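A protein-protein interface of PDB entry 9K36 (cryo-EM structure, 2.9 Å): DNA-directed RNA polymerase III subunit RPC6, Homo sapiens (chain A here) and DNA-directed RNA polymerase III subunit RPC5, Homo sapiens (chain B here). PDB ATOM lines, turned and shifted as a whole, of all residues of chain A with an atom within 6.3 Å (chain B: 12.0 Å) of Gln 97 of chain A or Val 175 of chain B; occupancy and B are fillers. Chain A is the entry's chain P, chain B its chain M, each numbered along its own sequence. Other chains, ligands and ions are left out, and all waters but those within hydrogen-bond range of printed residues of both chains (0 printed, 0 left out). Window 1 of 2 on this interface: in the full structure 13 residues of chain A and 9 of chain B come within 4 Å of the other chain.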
ATOM      1  N   ASP A  64      18.409  -1.964   8.325  1.00  0.00           N
ATOM      2  CA  ASP A  64      19.753  -2.495   8.173  1.00  0.00           C
ATOM      3  C   ASP A  64      20.595  -2.070   9.368  1.00  0.00           C
ATOM      4  O   ASP A  64      20.410  -0.984   9.927  1.00  0.00           O
ATOM      5  CB  ASP A  64      20.409  -2.011   6.872  1.00  0.00           C
ATOM      6  CG  ASP A  64      19.688  -2.511   5.636  1.00  0.00           C
ATOM      7  OD1 ASP A  64      19.156  -3.640   5.670  1.00  0.00           O
ATOM      8  OD2 ASP A  64      19.652  -1.774   4.627  1.00  0.00           O
ATOM      9  N   LYS A  77      16.064   0.971   5.028  1.00  0.00           N
ATOM     10  CA  LYS A  77      16.570   0.442   3.770  1.00  0.00           C
ATOM     11  C   LYS A  77      16.234   1.387   2.624  1.00  0.00           C
ATOM     12  O   LYS A  77      15.162   1.998   2.595  1.00  0.00           O
ATOM     13  CB  LYS A  77      15.990  -0.947   3.508  1.00  0.00           C
ATOM     14  CG  LYS A  77      16.689  -1.715   2.399  1.00  0.00           C
ATOM     15  CD  LYS A  77      16.229  -3.162   2.360  1.00  0.00           C
ATOM     16  CE  LYS A  77      17.031  -3.967   1.349  1.00  0.00           C
ATOM     17  NZ  LYS A  77      16.644  -5.404   1.344  1.00  0.00           N
ATOM     18  N   GLU A  92      14.321  -3.941  -7.992  1.00  0.00           N
ATOM     19  CA  GLU A  92      15.107  -2.720  -8.125  1.00  0.00           C
ATOM     20  C   GLU A  92      16.138  -2.611  -7.011  1.00  0.00           C
ATOM     21  O   GLU A  92      17.334  -2.422  -7.271  1.00  0.00           O
ATOM     22  CB  GLU A  92      14.179  -1.506  -8.122  1.00  0.00           C
ATOM     23  CG  GLU A  92      14.899  -0.182  -8.262  1.00  0.00           C
ATOM     24  CD  GLU A  92      13.967   0.995  -8.098  1.00  0.00           C
ATOM     25  OE1 GLU A  92      13.110   0.958  -7.192  1.00  0.00           O
ATOM     26  OE2 GLU A  92      14.082   1.953  -8.884  1.00  0.00           O
ATOM     27  N   LYS A  93      15.697  -2.744  -5.757  1.00  0.00           N
ATOM     28  CA  LYS A  93      16.644  -2.682  -4.651  1.00  0.00           C
ATOM     29  C   LYS A  93      17.533  -3.921  -4.602  1.00  0.00           C
ATOM     30  O   LYS A  93      18.706  -3.819  -4.229  1.00  0.00           O
ATOM     31  CB  LYS A  93      15.905  -2.482  -3.324  1.00  0.00           C
ATOM     32  CG  LYS A  93      14.876  -3.545  -2.976  1.00  0.00           C
ATOM     33  CD  LYS A  93      15.454  -4.619  -2.065  1.00  0.00           C
ATOM     34  CE  LYS A  93      14.413  -5.672  -1.722  1.00  0.00           C
ATOM     35  NZ  LYS A  93      14.967  -6.733  -0.837  1.00  0.00           N
ATOM     36  N   LEU A  94      17.015  -5.081  -5.011  1.00  0.00           N
ATOM     37  CA  LEU A  94      17.775  -6.324  -5.043  1.00  0.00           C
ATOM     38  C   LEU A  94      18.733  -6.398  -6.225  1.00  0.00           C
ATOM     39  O   LEU A  94      19.287  -7.466  -6.490  1.00  0.00           O
ATOM     40  CB  LEU A  94      16.814  -7.516  -5.074  1.00  0.00           C
ATOM     41  CG  LEU A  94      17.308  -8.848  -4.510  1.00  0.00           C
ATOM     42  CD1 LEU A  94      17.565  -8.728  -3.016  1.00  0.00           C
ATOM     43  CD2 LEU A  94      16.309  -9.957  -4.804  1.00  0.00           C
ATOM     44  N   VAL A  95      18.854  -5.319  -6.988  1.00  0.00           N
ATOM     45  CA  VAL A  95      19.973  -5.113  -7.904  1.00  0.00           C
ATOM     46  C   VAL A  95      20.857  -3.956  -7.441  1.00  0.00           C
ATOM     47  O   VAL A  95      22.089  -4.077  -7.389  1.00  0.00           O
ATOM     48  CB  VAL A  95      19.473  -4.890  -9.348  1.00  0.00           C
ATOM     49  CG1 VAL A  95      20.639  -4.576 -10.269  1.00  0.00           C
ATOM     50  CG2 VAL A  95      18.723  -6.113  -9.841  1.00  0.00           C
ATOM     51  N   TYR A  96      20.236  -2.828  -7.080  1.00  0.00           N
ATOM     52  CA  TYR A  96      20.980  -1.668  -6.597  1.00  0.00           C
ATOM     53  C   TYR A  96      21.818  -1.993  -5.368  1.00  0.00           C
ATOM     54  O   TYR A  96      22.816  -1.311  -5.117  1.00  0.00           O
ATOM     55  CB  TYR A  96      20.010  -0.523  -6.291  1.00  0.00           C
ATOM     56  CG  TYR A  96      20.676   0.808  -6.006  1.00  0.00           C
ATOM     57  CD1 TYR A  96      20.953   1.202  -4.704  1.00  0.00           C
ATOM     58  CD2 TYR A  96      21.016   1.673  -7.038  1.00  0.00           C
ATOM     59  CE1 TYR A  96      21.558   2.417  -4.436  1.00  0.00           C
ATOM     60  CE2 TYR A  96      21.621   2.891  -6.780  1.00  0.00           C
ATOM     61  CZ  TYR A  96      21.890   3.258  -5.478  1.00  0.00           C
ATOM     62  OH  TYR A  96      22.490   4.466  -5.217  1.00  0.00           O
ATOM     63  N   GLN A  97      21.454  -3.037  -4.617  1.00  0.00           N
ATOM     64  CA  GLN A  97      22.217  -3.414  -3.434  1.00  0.00           C
ATOM     65  C   GLN A  97      23.663  -3.744  -3.788  1.00  0.00           C
ATOM     66  O   GLN A  97      24.595  -3.066  -3.339  1.00  0.00           O
ATOM     67  CB  GLN A  97      21.532  -4.598  -2.754  1.00  0.00           C
ATOM     68  CG  GLN A  97      21.938  -4.854  -1.325  1.00  0.00           C
ATOM     69  CD  GLN A  97      21.043  -5.882  -0.658  1.00  0.00           C
ATOM     70  OE1 GLN A  97      21.083  -7.066  -0.992  1.00  0.00           O
ATOM     71  NE2 GLN A  97      20.216  -5.427   0.275  1.00  0.00           N
ATOM     72  N   ILE A  98      23.877  -4.775  -4.609  1.00  0.00           N
ATOM     73  CA  ILE A  98      25.240  -5.111  -5.004  1.00  0.00           C
ATOM     74  C   ILE A  98      25.800  -4.107  -6.009  1.00  0.00           C
ATOM     75  O   ILE A  98      27.022  -3.962  -6.098  1.00  0.00           O
ATOM     76  CB  ILE A  98      25.304  -6.563  -5.521  1.00  0.00           C
ATOM     77  CG1 ILE A  98      25.144  -7.538  -4.351  1.00  0.00           C
ATOM     78  CG2 ILE A  98      26.608  -6.864  -6.244  1.00  0.00           C
ATOM     79  CD1 ILE A  98      25.179  -8.994  -4.759  1.00  0.00           C
ATOM     80  N   ILE A  99      24.951  -3.358  -6.724  1.00  0.00           N
ATOM     81  CA  ILE A  99      25.482  -2.242  -7.509  1.00  0.00           C
ATOM     82  C   ILE A  99      26.255  -1.284  -6.606  1.00  0.00           C
ATOM     83  O   ILE A  99      27.410  -0.931  -6.883  1.00  0.00           O
ATOM     84  CB  ILE A  99      24.351  -1.521  -8.265  1.00  0.00           C
ATOM     85  CG1 ILE A  99      23.861  -2.381  -9.432  1.00  0.00           C
ATOM     86  CG2 ILE A  99      24.823  -0.165  -8.763  1.00  0.00           C
ATOM     87  CD1 ILE A  99      22.849  -1.686 -10.317  1.00  0.00           C
ATOM     88  N   GLU A 100      25.639  -0.877  -5.493  1.00  0.00           N
ATOM     89  CA  GLU A 100      26.310   0.000  -4.538  1.00  0.00           C
ATOM     90  C   GLU A 100      27.468  -0.708  -3.848  1.00  0.00           C
ATOM     91  O   GLU A 100      28.515  -0.097  -3.600  1.00  0.00           O
ATOM     92  CB  GLU A 100      25.304   0.509  -3.504  1.00  0.00           C
ATOM     93  CG  GLU A 100      25.922   1.315  -2.374  1.00  0.00           C
ATOM     94  CD  GLU A 100      24.899   1.759  -1.351  1.00  0.00           C
ATOM     95  OE1 GLU A 100      23.702   1.444  -1.526  1.00  0.00           O
ATOM     96  OE2 GLU A 100      25.290   2.425  -0.369  1.00  0.00           O
ATOM     97  N   ASP A 101      27.299  -1.994  -3.523  1.00  0.00           N
ATOM     98  CA  ASP A 101      28.375  -2.750  -2.887  1.00  0.00           C
ATOM     99  C   ASP A 101      29.634  -2.746  -3.746  1.00  0.00           C
ATOM    100  O   ASP A 101      30.750  -2.618  -3.228  1.00  0.00           O
ATOM    101  CB  ASP A 101      27.920  -4.182  -2.609  1.00  0.00           C
ATOM    102  CG  ASP A 101      26.801  -4.250  -1.589  1.00  0.00           C
ATOM    103  OD1 ASP A 101      26.745  -3.370  -0.704  1.00  0.00           O
ATOM    104  OD2 ASP A 101      25.974  -5.184  -1.670  1.00  0.00           O
ATOM    105  N   ALA A 102      29.476  -2.895  -5.063  1.00  0.00           N
ATOM    106  CA  ALA A 102      30.610  -2.751  -5.968  1.00  0.00           C
ATOM    107  C   ALA A 102      31.113  -1.313  -5.972  1.00  0.00           C
ATOM    108  O   ALA A 102      32.291  -1.054  -5.697  1.00  0.00           O
ATOM    109  CB  ALA A 102      30.220  -3.195  -7.378  1.00  0.00           C
ATOM    110  N   VAL B 170      34.578  -1.922  11.131  1.00  0.00           N
ATOM    111  CA  VAL B 170      33.184  -1.550  10.934  1.00  0.00           C
ATOM    112  C   VAL B 170      32.545  -2.524   9.958  1.00  0.00           C
ATOM    113  O   VAL B 170      33.118  -2.850   8.912  1.00  0.00           O
ATOM    114  CB  VAL B 170      33.079  -0.098  10.443  1.00  0.00           C
ATOM    115  CG1 VAL B 170      33.409   0.867  11.575  1.00  0.00           C
ATOM    116  CG2 VAL B 170      34.004   0.141   9.257  1.00  0.00           C
ATOM    117  N   LYS B 171      31.352  -3.007  10.305  1.00  0.00           N
ATOM    118  CA  LYS B 171      30.688  -3.984   9.453  1.00  0.00           C
ATOM    119  C   LYS B 171      30.171  -3.323   8.184  1.00  0.00           C
ATOM    120  O   LYS B 171      29.080  -2.742   8.178  1.00  0.00           O
ATOM    121  CB  LYS B 171      29.541  -4.671  10.197  1.00  0.00           C
ATOM    122  CG  LYS B 171      29.985  -5.602  11.315  1.00  0.00           C
ATOM    123  CD  LYS B 171      29.028  -6.778  11.461  1.00  0.00           C
ATOM    124  CE  LYS B 171      27.603  -6.318  11.724  1.00  0.00           C
ATOM    125  NZ  LYS B 171      27.466  -5.638  13.040  1.00  0.00           N
ATOM    126  N   GLN B 172      30.964  -3.387   7.113  1.00  0.00           N
ATOM    127  CA  GLN B 172      30.499  -2.962   5.800  1.00  0.00           C
ATOM    128  C   GLN B 172      29.191  -3.664   5.467  1.00  0.00           C
ATOM    129  O   GLN B 172      28.954  -4.799   5.889  1.00  0.00           O
ATOM    130  CB  GLN B 172      31.559  -3.271   4.739  1.00  0.00           C
ATOM    131  CG  GLN B 172      31.248  -2.726   3.353  1.00  0.00           C
ATOM    132  CD  GLN B 172      32.274  -3.149   2.320  1.00  0.00           C
ATOM    133  OE1 GLN B 172      33.238  -3.847   2.636  1.00  0.00           O
ATOM    134  NE2 GLN B 172      32.072  -2.728   1.079  1.00  0.00           N
ATOM    135  N   ILE B 173      28.340  -2.989   4.700  1.00  0.00           N
ATOM    136  CA  ILE B 173      26.988  -3.492   4.496  1.00  0.00           C
ATOM    137  C   ILE B 173      27.055  -4.658   3.522  1.00  0.00           C
ATOM    138  O   ILE B 173      27.043  -4.468   2.301  1.00  0.00           O
ATOM    139  CB  ILE B 173      26.050  -2.386   3.983  1.00  0.00           C
ATOM    140  CG1 ILE B 173      26.425  -1.041   4.606  1.00  0.00           C
ATOM    141  CG2 ILE B 173      24.605  -2.722   4.305  1.00  0.00           C
ATOM    142  CD1 ILE B 173      25.579   0.113   4.120  1.00  0.00           C
ATOM    143  N   THR B 174      27.134  -5.869   4.065  1.00  0.00           N
ATOM    144  CA  THR B 174      27.191  -7.093   3.267  1.00  0.00           C
ATOM    145  C   THR B 174      25.815  -7.739   3.147  1.00  0.00           C
ATOM    146  O   THR B 174      25.638  -8.931   3.401  1.00  0.00           O
ATOM    147  CB  THR B 174      28.200  -8.063   3.867  1.00  0.00           C
ATOM    148  OG1 THR B 174      27.809  -8.393   5.207  1.00  0.00           O
ATOM    149  CG2 THR B 174      29.591  -7.442   3.888  1.00  0.00           C
ATOM    150  N   VAL B 175      24.826  -6.942   2.754  1.00  0.00           N
ATOM    151  CA  VAL B 175      23.479  -7.461   2.542  1.00  0.00           C
ATOM    152  C   VAL B 175      23.456  -8.219   1.222  1.00  0.00           C
ATOM    153  O   VAL B 175      23.596  -7.629   0.143  1.00  0.00           O
ATOM    154  CB  VAL B 175      22.446  -6.328   2.560  1.00  0.00           C
ATOM    155  CG1 VAL B 175      21.916  -6.122   3.972  1.00  0.00           C
ATOM    156  CG2 VAL B 175      23.066  -5.043   2.037  1.00  0.00           C
ATOM    157  N   ARG B 176      23.291  -9.536   1.302  1.00  0.00           N
ATOM    158  CA  ARG B 176      23.343 -10.391   0.129  1.00  0.00           C
ATOM    159  C   ARG B 176      22.006 -10.393  -0.602  1.00  0.00           C
ATOM    160  O   ARG B 176      20.946 -10.188  -0.004  1.00  0.00           O
ATOM    161  CB  ARG B 176      23.722 -11.822   0.513  1.00  0.00           C
ATOM    162  CG  ARG B 176      25.149 -11.984   1.005  1.00  0.00           C
ATOM    163  CD  ARG B 176      25.470 -13.449   1.252  1.00  0.00           C
ATOM    164  NE  ARG B 176      26.878 -13.663   1.566  1.00  0.00           N
ATOM    165  CZ  ARG B 176      27.425 -14.861   1.754  1.00  0.00           C
ATOM    166  NH1 ARG B 176      26.680 -15.952   1.658  1.00  0.00           N
ATOM    167  NH2 ARG B 176      28.716 -14.966   2.035  1.00  0.00           N
ATOM    168  N   PHE B 177      22.073 -10.619  -1.911  1.00  0.00           N
ATOM    169  CA  PHE B 177      20.866 -10.748  -2.715  1.00  0.00           C
ATOM    170  C   PHE B 177      20.039 -11.934  -2.245  1.00  0.00           C
ATOM    171  O   PHE B 177      20.554 -13.047  -2.098  1.00  0.00           O
ATOM    172  CB  PHE B 177      21.227 -10.924  -4.193  1.00  0.00           C
ATOM    173  CG  PHE B 177      21.566  -9.644  -4.898  1.00  0.00           C
ATOM    174  CD1 PHE B 177      21.468  -8.427  -4.248  1.00  0.00           C
ATOM    175  CD2 PHE B 177      21.967  -9.661  -6.224  1.00  0.00           C
ATOM    176  CE1 PHE B 177      21.777  -7.254  -4.906  1.00  0.00           C
ATOM    177  CE2 PHE B 177      22.274  -8.493  -6.885  1.00  0.00           C
ATOM    178  CZ  PHE B 177      22.176  -7.286  -6.229  1.00  0.00           C
ATOM    179  N   SER B 178      18.750 -11.696  -2.010  1.00  0.00           N
ATOM    180  CA  SER B 178      17.803 -12.787  -1.786  1.00  0.00           C
ATOM    181  C   SER B 178      17.510 -13.408  -3.147  1.00  0.00           C
ATOM    182  O   SER B 178      16.460 -13.198  -3.757  1.00  0.00           O
ATOM    183  CB  SER B 178      16.538 -12.283  -1.102  1.00  0.00           C
ATOM    184  OG  SER B 178      15.860 -11.340  -1.914  1.00  0.00           O
ATOM    185  N   ARG B 179      18.483 -14.173  -3.636  1.00  0.00           N
ATOM    186  CA  ARG B 179      18.412 -14.723  -4.983  1.00  0.00           C
ATOM    187  C   ARG B 179      17.196 -15.633  -5.118  1.00  0.00           C
ATOM    188  O   ARG B 179      16.899 -16.402  -4.193  1.00  0.00           O
ATOM    189  CB  ARG B 179      19.681 -15.507  -5.313  1.00  0.00           C
ATOM    190  CG  ARG B 179      20.970 -14.710  -5.233  1.00  0.00           C
ATOM    191  CD  ARG B 179      22.162 -15.581  -5.597  1.00  0.00           C
ATOM    192  NE  ARG B 179      23.427 -14.857  -5.522  1.00  0.00           N
ATOM    193  CZ  ARG B 179      24.612 -15.396  -5.792  1.00  0.00           C
ATOM    194  NH1 ARG B 179      24.696 -16.668  -6.157  1.00  0.00           N
ATOM    195  NH2 ARG B 179      25.713 -14.663  -5.696  1.00  0.00           N
ATOM    196  N   PRO B 180      16.469 -15.574  -6.232  1.00  0.00           N
ATOM    197  CA  PRO B 180      15.395 -16.549  -6.452  1.00  0.00           C
ATOM    198  C   PRO B 180      15.966 -17.951  -6.576  1.00  0.00           C
ATOM    199  O   PRO B 180      16.640 -18.277  -7.561  1.00  0.00           O
ATOM    200  CB  PRO B 180      14.747 -16.075  -7.759  1.00  0.00           C
ATOM    201  CG  PRO B 180      15.815 -15.286  -8.448  1.00  0.00           C
ATOM    202  CD  PRO B 180      16.604 -14.629  -7.354  1.00  0.00           C
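The side-chain amide oxygen of Gln 97 of chain A lies close to the backbone carbonyl oxygen of Val 175 of chain B, 2.8 Å away. The backbone carbonyl oxygen (O) of Arg 176 of chain B sits close to the side-chain amide oxygen (OE1) of Gln 97 of chain A. The side-chain carboxylate of Asp 101 of chain A sits close to the backbone carbonyl oxygen of Ile 173 of chain B, at 3.2 Å.
Of the 11 printed residues of chain B, 5 touch a printed residue of chain A. Hydrophobic or aromatic side chains of chain B that line the printed part of chain A: Val 175 and Phe 177. Printed residues of chain A that touch a printed residue of chain B: Leu 94, Val 95, Gln 97, Ile 98 and Asp 101. Hydrophobic or aromatic side chains of chain A within 4 Å of the printed part of chain B: Leu 94 and Ile 98. Among the printed residues, no Asp or Glu carboxylate lies within 4 Å of a Lys or Arg side-chain nitrogen of the other chain.
Of chain B, only Val 175 (2.8 Å), Arg 176 (3.3 Å) and Phe 177 (3.4 Å) come within 4 Å of Gln 97 of chain A. No residue of chain B comes within 4 Å of Lys 93 of chain A. Of chain B, only Phe 177 and Ser 178 come within 4 Å of Leu 94 of chain A. No residue of chain B comes within 4 Å of Tyr 96 of chain A. Ile 98 of chain A touches just one residue of chain B: Phe 177. No residue of chain B comes within 4 Å of Ile 99 of chain A. No residue of chain B comes within 4 Å of Glu 100 of chain A. Of chain B, only Ile 173 and Val 175 come within 4 Å of Asp 101 of chain A. Printed residues of chain A within 4 Å of Ser 178 of chain B: Leu 94 (3.2 Å). Of the printed residues of chain A, Phe 177 of chain B touches Leu 94 (2.9 Å), Val 95 (3.4 Å), Gln 97 (3.4 Å) and Ile 98 (3.3 Å). Asp 64 of chain A touches none of the printed residues of chain B. Lys 171 of chain B touches none of the printed residues of chain A. The nearest residue of chain B that does not touch Gln 97 of chain A is Ser 178 of chain B (5.3 Å). The nearest residue of chain A that does not touch Val 175 of chain B is Asp 64 of chain A (4.1 Å). The nearest printed residue of chain A that does not touch Phe 177 of chain B is Lys 93 of chain A (4.7 Å).
Among the printed residues, pairs that only touch across the chains: Leu 94 of chain A with Phe 177 of chain B, Leu 94 of chain A with Ser 178 of chain B, Val 95 of chain A with Phe 177 of chain B, Gln 97 of chain A with Phe 177 of chain B, Ile 98 of chain A with Phe 177 of chain B and Asp 101 of chain A with Val 175 of chain B.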
